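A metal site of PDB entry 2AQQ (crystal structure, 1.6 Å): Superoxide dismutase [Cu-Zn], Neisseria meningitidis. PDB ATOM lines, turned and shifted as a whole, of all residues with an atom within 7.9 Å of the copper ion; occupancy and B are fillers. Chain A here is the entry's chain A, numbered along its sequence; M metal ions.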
ATOM      1  N   GLY A  55      19.864  22.342 -23.193  1.00  0.00           N
ATOM      2  CA  GLY A  55      20.651  21.907 -24.344  1.00  0.00           C
ATOM      3  C   GLY A  55      20.751  20.395 -24.233  1.00  0.00           C
ATOM      4  O   GLY A  55      21.025  19.867 -23.160  1.00  0.00           O
ATOM      5  N   PHE A  56      20.580  19.715 -25.360  1.00  0.00           N
ATOM      6  CA  PHE A  56      20.563  18.260 -25.403  1.00  0.00           C
ATOM      7  C   PHE A  56      21.337  17.843 -26.660  1.00  0.00           C
ATOM      8  O   PHE A  56      20.867  18.048 -27.771  1.00  0.00           O
ATOM      9  CB  PHE A  56      19.084  17.860 -25.500  1.00  0.00           C
ATOM     10  CG  PHE A  56      18.784  16.422 -25.162  1.00  0.00           C
ATOM     11  CD1 PHE A  56      19.437  15.769 -24.111  1.00  0.00           C
ATOM     12  CD2 PHE A  56      17.775  15.749 -25.840  1.00  0.00           C
ATOM     13  CE1 PHE A  56      19.058  14.483 -23.742  1.00  0.00           C
ATOM     14  CE2 PHE A  56      17.389  14.463 -25.477  1.00  0.00           C
ATOM     15  CZ  PHE A  56      18.035  13.827 -24.418  1.00  0.00           C
ATOM     16  N   HIS A  57      22.529  17.288 -26.475  1.00  0.00           N
ATOM     17  CA  HIS A  57      23.349  16.885 -27.618  1.00  0.00           C
ATOM     18  C   HIS A  57      24.154  15.608 -27.410  1.00  0.00           C
ATOM     19  O   HIS A  57      24.420  15.202 -26.280  1.00  0.00           O
ATOM     20  CB  HIS A  57      24.360  17.974 -27.995  1.00  0.00           C
ATOM     21  CG  HIS A  57      23.986  19.350 -27.557  1.00  0.00           C
ATOM     22  ND1 HIS A  57      24.605  19.986 -26.498  1.00  0.00           N
ATOM     23  CD2 HIS A  57      23.078  20.226 -28.045  1.00  0.00           C
ATOM     24  CE1 HIS A  57      24.086  21.193 -26.351  1.00  0.00           C
ATOM     25  NE2 HIS A  57      23.153  21.359 -27.271  1.00  0.00           N
ATOM     26  N   ILE A  58      24.553  14.996 -28.518  1.00  0.00           N
ATOM     27  CA  ILE A  58      25.394  13.807 -28.455  1.00  0.00           C
ATOM     28  C   ILE A  58      26.807  14.390 -28.462  1.00  0.00           C
ATOM     29  O   ILE A  58      27.105  15.239 -29.303  1.00  0.00           O
ATOM     30  CB  ILE A  58      25.270  12.925 -29.713  1.00  0.00           C
ATOM     31  CG1 ILE A  58      23.807  12.481 -29.906  1.00  0.00           C
ATOM     32  CG2 ILE A  58      26.209  11.715 -29.596  1.00  0.00           C
ATOM     33  CD1 ILE A  58      23.255  11.657 -28.762  1.00  0.00           C
ATOM     34  N   HIS A  59      27.653  13.973 -27.521  1.00  0.00           N
ATOM     35  CA  HIS A  59      29.026  14.458 -27.499  1.00  0.00           C
ATOM     36  C   HIS A  59      29.925  13.336 -28.014  1.00  0.00           C
ATOM     37  O   HIS A  59      29.548  12.156 -27.964  1.00  0.00           O
ATOM     38  CB  HIS A  59      29.426  14.922 -26.103  1.00  0.00           C
ATOM     39  CG  HIS A  59      28.900  16.285 -25.765  1.00  0.00           C
ATOM     40  ND1 HIS A  59      29.721  17.329 -25.385  1.00  0.00           N
ATOM     41  CD2 HIS A  59      27.642  16.785 -25.802  1.00  0.00           C
ATOM     42  CE1 HIS A  59      28.991  18.415 -25.196  1.00  0.00           C
ATOM     43  NE2 HIS A  59      27.725  18.114 -25.443  1.00  0.00           N
ATOM     44  N   ALA A  79      33.688  14.118 -21.966  1.00  0.00           N
ATOM     45  CA  ALA A  79      32.833  13.755 -23.086  1.00  0.00           C
ATOM     46  C   ALA A  79      33.273  14.422 -24.391  1.00  0.00           C
ATOM     47  O   ALA A  79      32.866  14.028 -25.476  1.00  0.00           O
ATOM     48  CB  ALA A  79      31.389  14.121 -22.792  1.00  0.00           C
ATOM     49  N   GLY A  80      34.122  15.440 -24.269  1.00  0.00           N
ATOM     50  CA  GLY A  80      34.570  16.142 -25.462  1.00  0.00           C
ATOM     51  C   GLY A  80      33.512  17.116 -25.961  1.00  0.00           C
ATOM     52  O   GLY A  80      32.593  17.473 -25.219  1.00  0.00           O
ATOM     53  N   GLY A  81      33.624  17.524 -27.216  1.00  0.00           N
ATOM     54  CA  GLY A  81      32.669  18.468 -27.770  1.00  0.00           C
ATOM     55  C   GLY A  81      31.464  17.813 -28.392  1.00  0.00           C
ATOM     56  O   GLY A  81      31.248  16.603 -28.268  1.00  0.00           O
ATOM     57  N   HIS A  82      30.647  18.612 -29.075  1.00  0.00           N
ATOM     58  CA  HIS A  82      29.457  18.079 -29.728  1.00  0.00           C
ATOM     59  C   HIS A  82      29.934  17.114 -30.807  1.00  0.00           C
ATOM     60  O   HIS A  82      30.890  17.407 -31.523  1.00  0.00           O
ATOM     61  CB  HIS A  82      28.654  19.204 -30.378  1.00  0.00           C
ATOM     62  CG  HIS A  82      28.032  20.155 -29.392  1.00  0.00           C
ATOM     63  ND1 HIS A  82      26.997  21.001 -29.737  1.00  0.00           N
ATOM     64  CD2 HIS A  82      28.299  20.390 -28.090  1.00  0.00           C
ATOM     65  CE1 HIS A  82      26.667  21.735 -28.690  1.00  0.00           C
ATOM     66  NE2 HIS A  82      27.434  21.384 -27.675  1.00  0.00           N
ATOM     67  N   TRP A  83      29.275  15.968 -30.920  1.00  0.00           N
ATOM     68  CA  TRP A  83      29.664  14.997 -31.928  1.00  0.00           C
ATOM     69  C   TRP A  83      29.504  15.634 -33.311  1.00  0.00           C
ATOM     70  O   TRP A  83      28.411  16.050 -33.700  1.00  0.00           O
ATOM     71  CB  TRP A  83      28.808  13.743 -31.805  1.00  0.00           C
ATOM     72  CG  TRP A  83      29.295  12.624 -32.655  1.00  0.00           C
ATOM     73  CD1 TRP A  83      30.599  12.247 -32.835  1.00  0.00           C
ATOM     74  CD2 TRP A  83      28.503  11.735 -33.445  1.00  0.00           C
ATOM     75  NE1 TRP A  83      30.656  11.168 -33.697  1.00  0.00           N
ATOM     76  CE2 TRP A  83      29.386  10.843 -34.075  1.00  0.00           C
ATOM     77  CE3 TRP A  83      27.125  11.614 -33.669  1.00  0.00           C
ATOM     78  CZ2 TRP A  83      28.938   9.821 -34.924  1.00  0.00           C
ATOM     79  CZ3 TRP A  83      26.674  10.601 -34.514  1.00  0.00           C
ATOM     80  CH2 TRP A  83      27.582   9.722 -35.127  1.00  0.00           C
ATOM     81  N   HIS A  91      27.334  24.857 -34.590  1.00  0.00           N
ATOM     82  CA  HIS A  91      26.190  24.359 -33.830  1.00  0.00           C
ATOM     83  C   HIS A  91      24.915  24.868 -34.511  1.00  0.00           C
ATOM     84  O   HIS A  91      24.849  26.033 -34.906  1.00  0.00           O
ATOM     85  CB  HIS A  91      26.241  24.844 -32.388  1.00  0.00           C
ATOM     86  CG  HIS A  91      25.114  24.337 -31.541  1.00  0.00           C
ATOM     87  ND1 HIS A  91      24.994  23.007 -31.193  1.00  0.00           N
ATOM     88  CD2 HIS A  91      24.030  24.964 -31.032  1.00  0.00           C
ATOM     89  CE1 HIS A  91      23.885  22.841 -30.500  1.00  0.00           C
ATOM     90  NE2 HIS A  91      23.277  24.006 -30.388  1.00  0.00           N
ATOM     91  N   GLY A 102      25.443  15.797 -33.804  1.00  0.00           N
ATOM     92  CA  GLY A 102      24.973  15.516 -32.460  1.00  0.00           C
ATOM     93  C   GLY A 102      23.954  16.493 -31.900  1.00  0.00           C
ATOM     94  O   GLY A 102      23.522  16.340 -30.764  1.00  0.00           O
ATOM     95  N   ASP A 103      23.564  17.486 -32.686  1.00  0.00           N
ATOM     96  CA  ASP A 103      22.605  18.487 -32.210  1.00  0.00           C
ATOM     97  C   ASP A 103      21.171  17.962 -32.193  1.00  0.00           C
ATOM     98  O   ASP A 103      20.554  17.746 -33.234  1.00  0.00           O
ATOM     99  CB  ASP A 103      22.702  19.756 -33.075  1.00  0.00           C
ATOM    100  CG  ASP A 103      24.048  20.454 -32.929  1.00  0.00           C
ATOM    101  OD1 ASP A 103      24.772  20.139 -31.955  1.00  0.00           O
ATOM    102  OD2 ASP A 103      24.369  21.322 -33.766  1.00  0.00           O
ATOM    103  N   SER A 134      28.308   9.913 -26.071  1.00  0.00           N
ATOM    104  CA  SER A 134      27.602  10.289 -24.847  1.00  0.00           C
ATOM    105  C   SER A 134      26.459  11.225 -25.173  1.00  0.00           C
ATOM    106  O   SER A 134      26.417  11.837 -26.237  1.00  0.00           O
ATOM    107  CB  SER A 134      28.579  10.960 -23.875  1.00  0.00           C
ATOM    108  OG  SER A 134      29.336  11.968 -24.524  1.00  0.00           O
ATOM    109  N   ILE A 135      25.493  11.316 -24.261  1.00  0.00           N
ATOM    110  CA  ILE A 135      24.366  12.224 -24.456  1.00  0.00           C
ATOM    111  C   ILE A 135      24.466  13.195 -23.290  1.00  0.00           C
ATOM    112  O   ILE A 135      24.584  12.800 -22.129  1.00  0.00           O
ATOM    113  CB  ILE A 135      23.018  11.467 -24.495  1.00  0.00           C
ATOM    114  CG1 ILE A 135      21.888  12.447 -24.806  1.00  0.00           C
ATOM    115  CG2 ILE A 135      22.774  10.721 -23.185  1.00  0.00           C
ATOM    116  CD1 ILE A 135      20.677  11.786 -25.421  1.00  0.00           C
ATOM    117  N   MET A 136      24.438  14.478 -23.607  1.00  0.00           N
ATOM    118  CA  MET A 136      24.609  15.527 -22.611  1.00  0.00           C
ATOM    119  C   MET A 136      23.403  16.430 -22.415  1.00  0.00           C
ATOM    120  O   MET A 136      22.726  16.782 -23.381  1.00  0.00           O
ATOM    121  CB  MET A 136      25.802  16.391 -23.030  1.00  0.00           C
ATOM    122  CG  MET A 136      26.357  17.297 -21.957  1.00  0.00           C
ATOM    123  SD  MET A 136      27.355  16.381 -20.771  1.00  0.00           S
ATOM    124  CE  MET A 136      28.669  15.763 -21.841  1.00  0.00           C
ATOM    125  N   ILE A 137      23.161  16.799 -21.170  1.00  0.00           N
ATOM    126  CA  ILE A 137      22.069  17.716 -20.830  1.00  0.00           C
ATOM    127  C   ILE A 137      22.760  18.899 -20.165  1.00  0.00           C
ATOM    128  O   ILE A 137      23.433  18.741 -19.146  1.00  0.00           O
ATOM    129  CB  ILE A 137      21.065  17.078 -19.868  1.00  0.00           C
ATOM    130  CG1 ILE A 137      20.404  15.874 -20.537  1.00  0.00           C
ATOM    131  CG2 ILE A 137      20.018  18.114 -19.442  1.00  0.00           C
ATOM    132  CD1 ILE A 137      19.527  15.037 -19.615  1.00  0.00           C
ATOM    133  N   HIS A 138      22.608  20.078 -20.750  1.00  0.00           N
ATOM    134  CA  HIS A 138      23.246  21.266 -20.221  1.00  0.00           C
ATOM    135  C   HIS A 138      22.390  22.034 -19.229  1.00  0.00           C
ATOM    136  O   HIS A 138      21.190  21.831 -19.141  1.00  0.00           O
ATOM    137  CB  HIS A 138      23.644  22.180 -21.386  1.00  0.00           C
ATOM    138  CG  HIS A 138      24.715  21.602 -22.256  1.00  0.00           C
ATOM    139  ND1 HIS A 138      26.053  21.895 -22.090  1.00  0.00           N
ATOM    140  CD2 HIS A 138      24.653  20.705 -23.268  1.00  0.00           C
ATOM    141  CE1 HIS A 138      26.767  21.219 -22.966  1.00  0.00           C
ATOM    142  NE2 HIS A 138      25.949  20.479 -23.695  1.00  0.00           N
ATOM    143  N   ASP A 142      19.106  26.016 -25.511  1.00  0.00           N
ATOM    144  CA  ASP A 142      19.696  25.833 -26.829  1.00  0.00           C
ATOM    145  C   ASP A 142      18.959  26.671 -27.874  1.00  0.00           C
ATOM    146  O   ASP A 142      17.797  26.379 -28.208  1.00  0.00           O
ATOM    147  CB  ASP A 142      19.630  24.359 -27.239  1.00  0.00           C
ATOM    148  CG  ASP A 142      20.594  24.014 -28.364  1.00  0.00           C
ATOM    149  OD1 ASP A 142      21.027  24.943 -29.085  1.00  0.00           O
ATOM    150  OD2 ASP A 142      20.931  22.829 -28.532  1.00  0.00           O
ATOM    151  N   LEU A 151      27.679  27.299 -28.974  1.00  0.00           N
ATOM    152  CA  LEU A 151      26.977  26.054 -28.738  1.00  0.00           C
ATOM    153  C   LEU A 151      25.552  26.196 -28.181  1.00  0.00           C
ATOM    154  O   LEU A 151      25.148  25.448 -27.294  1.00  0.00           O
ATOM    155  CB  LEU A 151      27.832  25.186 -27.812  1.00  0.00           C
ATOM    156  CG  LEU A 151      29.277  25.050 -28.315  1.00  0.00           C
ATOM    157  CD1 LEU A 151      30.127  24.334 -27.292  1.00  0.00           C
ATOM    158  CD2 LEU A 151      29.291  24.305 -29.637  1.00  0.00           C
ATOM    159  N   GLY A 154      24.206  26.501 -24.179  1.00  0.00           N
ATOM    160  CA  GLY A 154      24.028  25.408 -23.234  1.00  0.00           C
ATOM    161  C   GLY A 154      24.858  25.612 -21.981  1.00  0.00           C
ATOM    162  O   GLY A 154      24.430  25.246 -20.882  1.00  0.00           O
ATOM    163  N   GLY A 155      26.046  26.176 -22.141  1.00  0.00           N
ATOM    164  CA  GLY A 155      26.899  26.399 -20.991  1.00  0.00           C
ATOM    165  C   GLY A 155      27.344  25.100 -20.330  1.00  0.00           C
ATOM    166  O   GLY A 155      27.580  24.103 -21.016  1.00  0.00           O
ATOM    167  N   PRO A 156      27.476  25.087 -19.000  1.00  0.00           N
ATOM    168  CA  PRO A 156      27.889  23.932 -18.196  1.00  0.00           C
ATOM    169  C   PRO A 156      27.118  22.648 -18.485  1.00  0.00           C
ATOM    170  O   PRO A 156      25.997  22.674 -18.984  1.00  0.00           O
ATOM    171  CB  PRO A 156      27.694  24.409 -16.762  1.00  0.00           C
ATOM    172  CG  PRO A 156      27.976  25.867 -16.869  1.00  0.00           C
ATOM    173  CD  PRO A 156      27.242  26.259 -18.133  1.00  0.00           C
ATOM    174  N   ARG A 157      27.732  21.530 -18.121  1.00  0.00           N
ATOM    175  CA  ARG A 157      27.124  20.211 -18.323  1.00  0.00           C
ATOM    176  C   ARG A 157      26.513  19.761 -17.003  1.00  0.00           C
ATOM    177  O   ARG A 157      27.214  19.548 -16.017  1.00  0.00           O
ATOM    178  CB  ARG A 157      28.202  19.257 -18.828  1.00  0.00           C
ATOM    179  CG  ARG A 157      28.834  19.808 -20.096  1.00  0.00           C
ATOM    180  CD  ARG A 157      29.993  19.001 -20.631  1.00  0.00           C
ATOM    181  NE  ARG A 157      30.571  19.696 -21.775  1.00  0.00           N
ATOM    182  CZ  ARG A 157      31.432  19.173 -22.634  1.00  0.00           C
ATOM    183  NH1 ARG A 157      31.832  17.912 -22.496  1.00  0.00           N
ATOM    184  NH2 ARG A 157      31.882  19.902 -23.649  1.00  0.00           N
ATOM    185  N   ALA A 159      23.876  17.044 -16.707  1.00  0.00           N
ATOM    186  CA  ALA A 159      23.646  15.611 -16.613  1.00  0.00           C
ATOM    187  C   ALA A 159      24.214  14.935 -17.852  1.00  0.00           C
ATOM    188  O   ALA A 159      24.369  15.566 -18.896  1.00  0.00           O
ATOM    189  CB  ALA A 159      22.151  15.324 -16.481  1.00  0.00           C
HETATM  190 CU    CU M   1      26.153  19.357 -25.388  1.00  0.00          CU
HETATM  191 ZN    ZN M   2      26.189  21.388 -31.581  1.00  0.00          ZN
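His 82 touches the copper ion. Met 136 touches the copper ion. Five residues have an atom within 4 Å of the copper ion: His 57, His 59, His 82, Met 136 and His 138. Along chain A the residues within 4 Å of the copper ion span positions 57 to 138.
The copper ion is bound by NE2 of His 59 (2.0 Å). A ring nitrogen (ND1) of His 57 is bound to the copper ion. The copper ion is bound by a ring nitrogen (NE2) of His 138, 2.0 Å away.
The backbone carbonyl oxygen (O) of Pro 156 is in hydrogen-bond range of a ring nitrogen (ND1) of His 138. A ring nitrogen (ND1) of His 59 sits close to the backbone carbonyl oxygen (O) of Gly 81, at 3.3 Å. The backbone NH (N) of His 138 lies within hydrogen-bond range of the backbone carbonyl oxygen (O) of Gly 55 (2.9 Å). A ring nitrogen (NE2) of His 57 lies within hydrogen-bond range of the side-chain carboxylate (OD2) of Asp 142 (2.9 Å). A ring nitrogen (ND1) of His 57 sits close to a ring nitrogen (NE2) of His 82, at 3.4 Å. The backbone NH (N) of His 59 lies within hydrogen-bond range of the backbone carbonyl oxygen (O) of Ser 134. The backbone carbonyl oxygen of His 57 sits at hydrogen-bond distance from the backbone NH of Met 136, 2.8 Å away. ND1 of His 138 is in hydrogen-bond range of O of Gly 155, at 2.9 Å.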
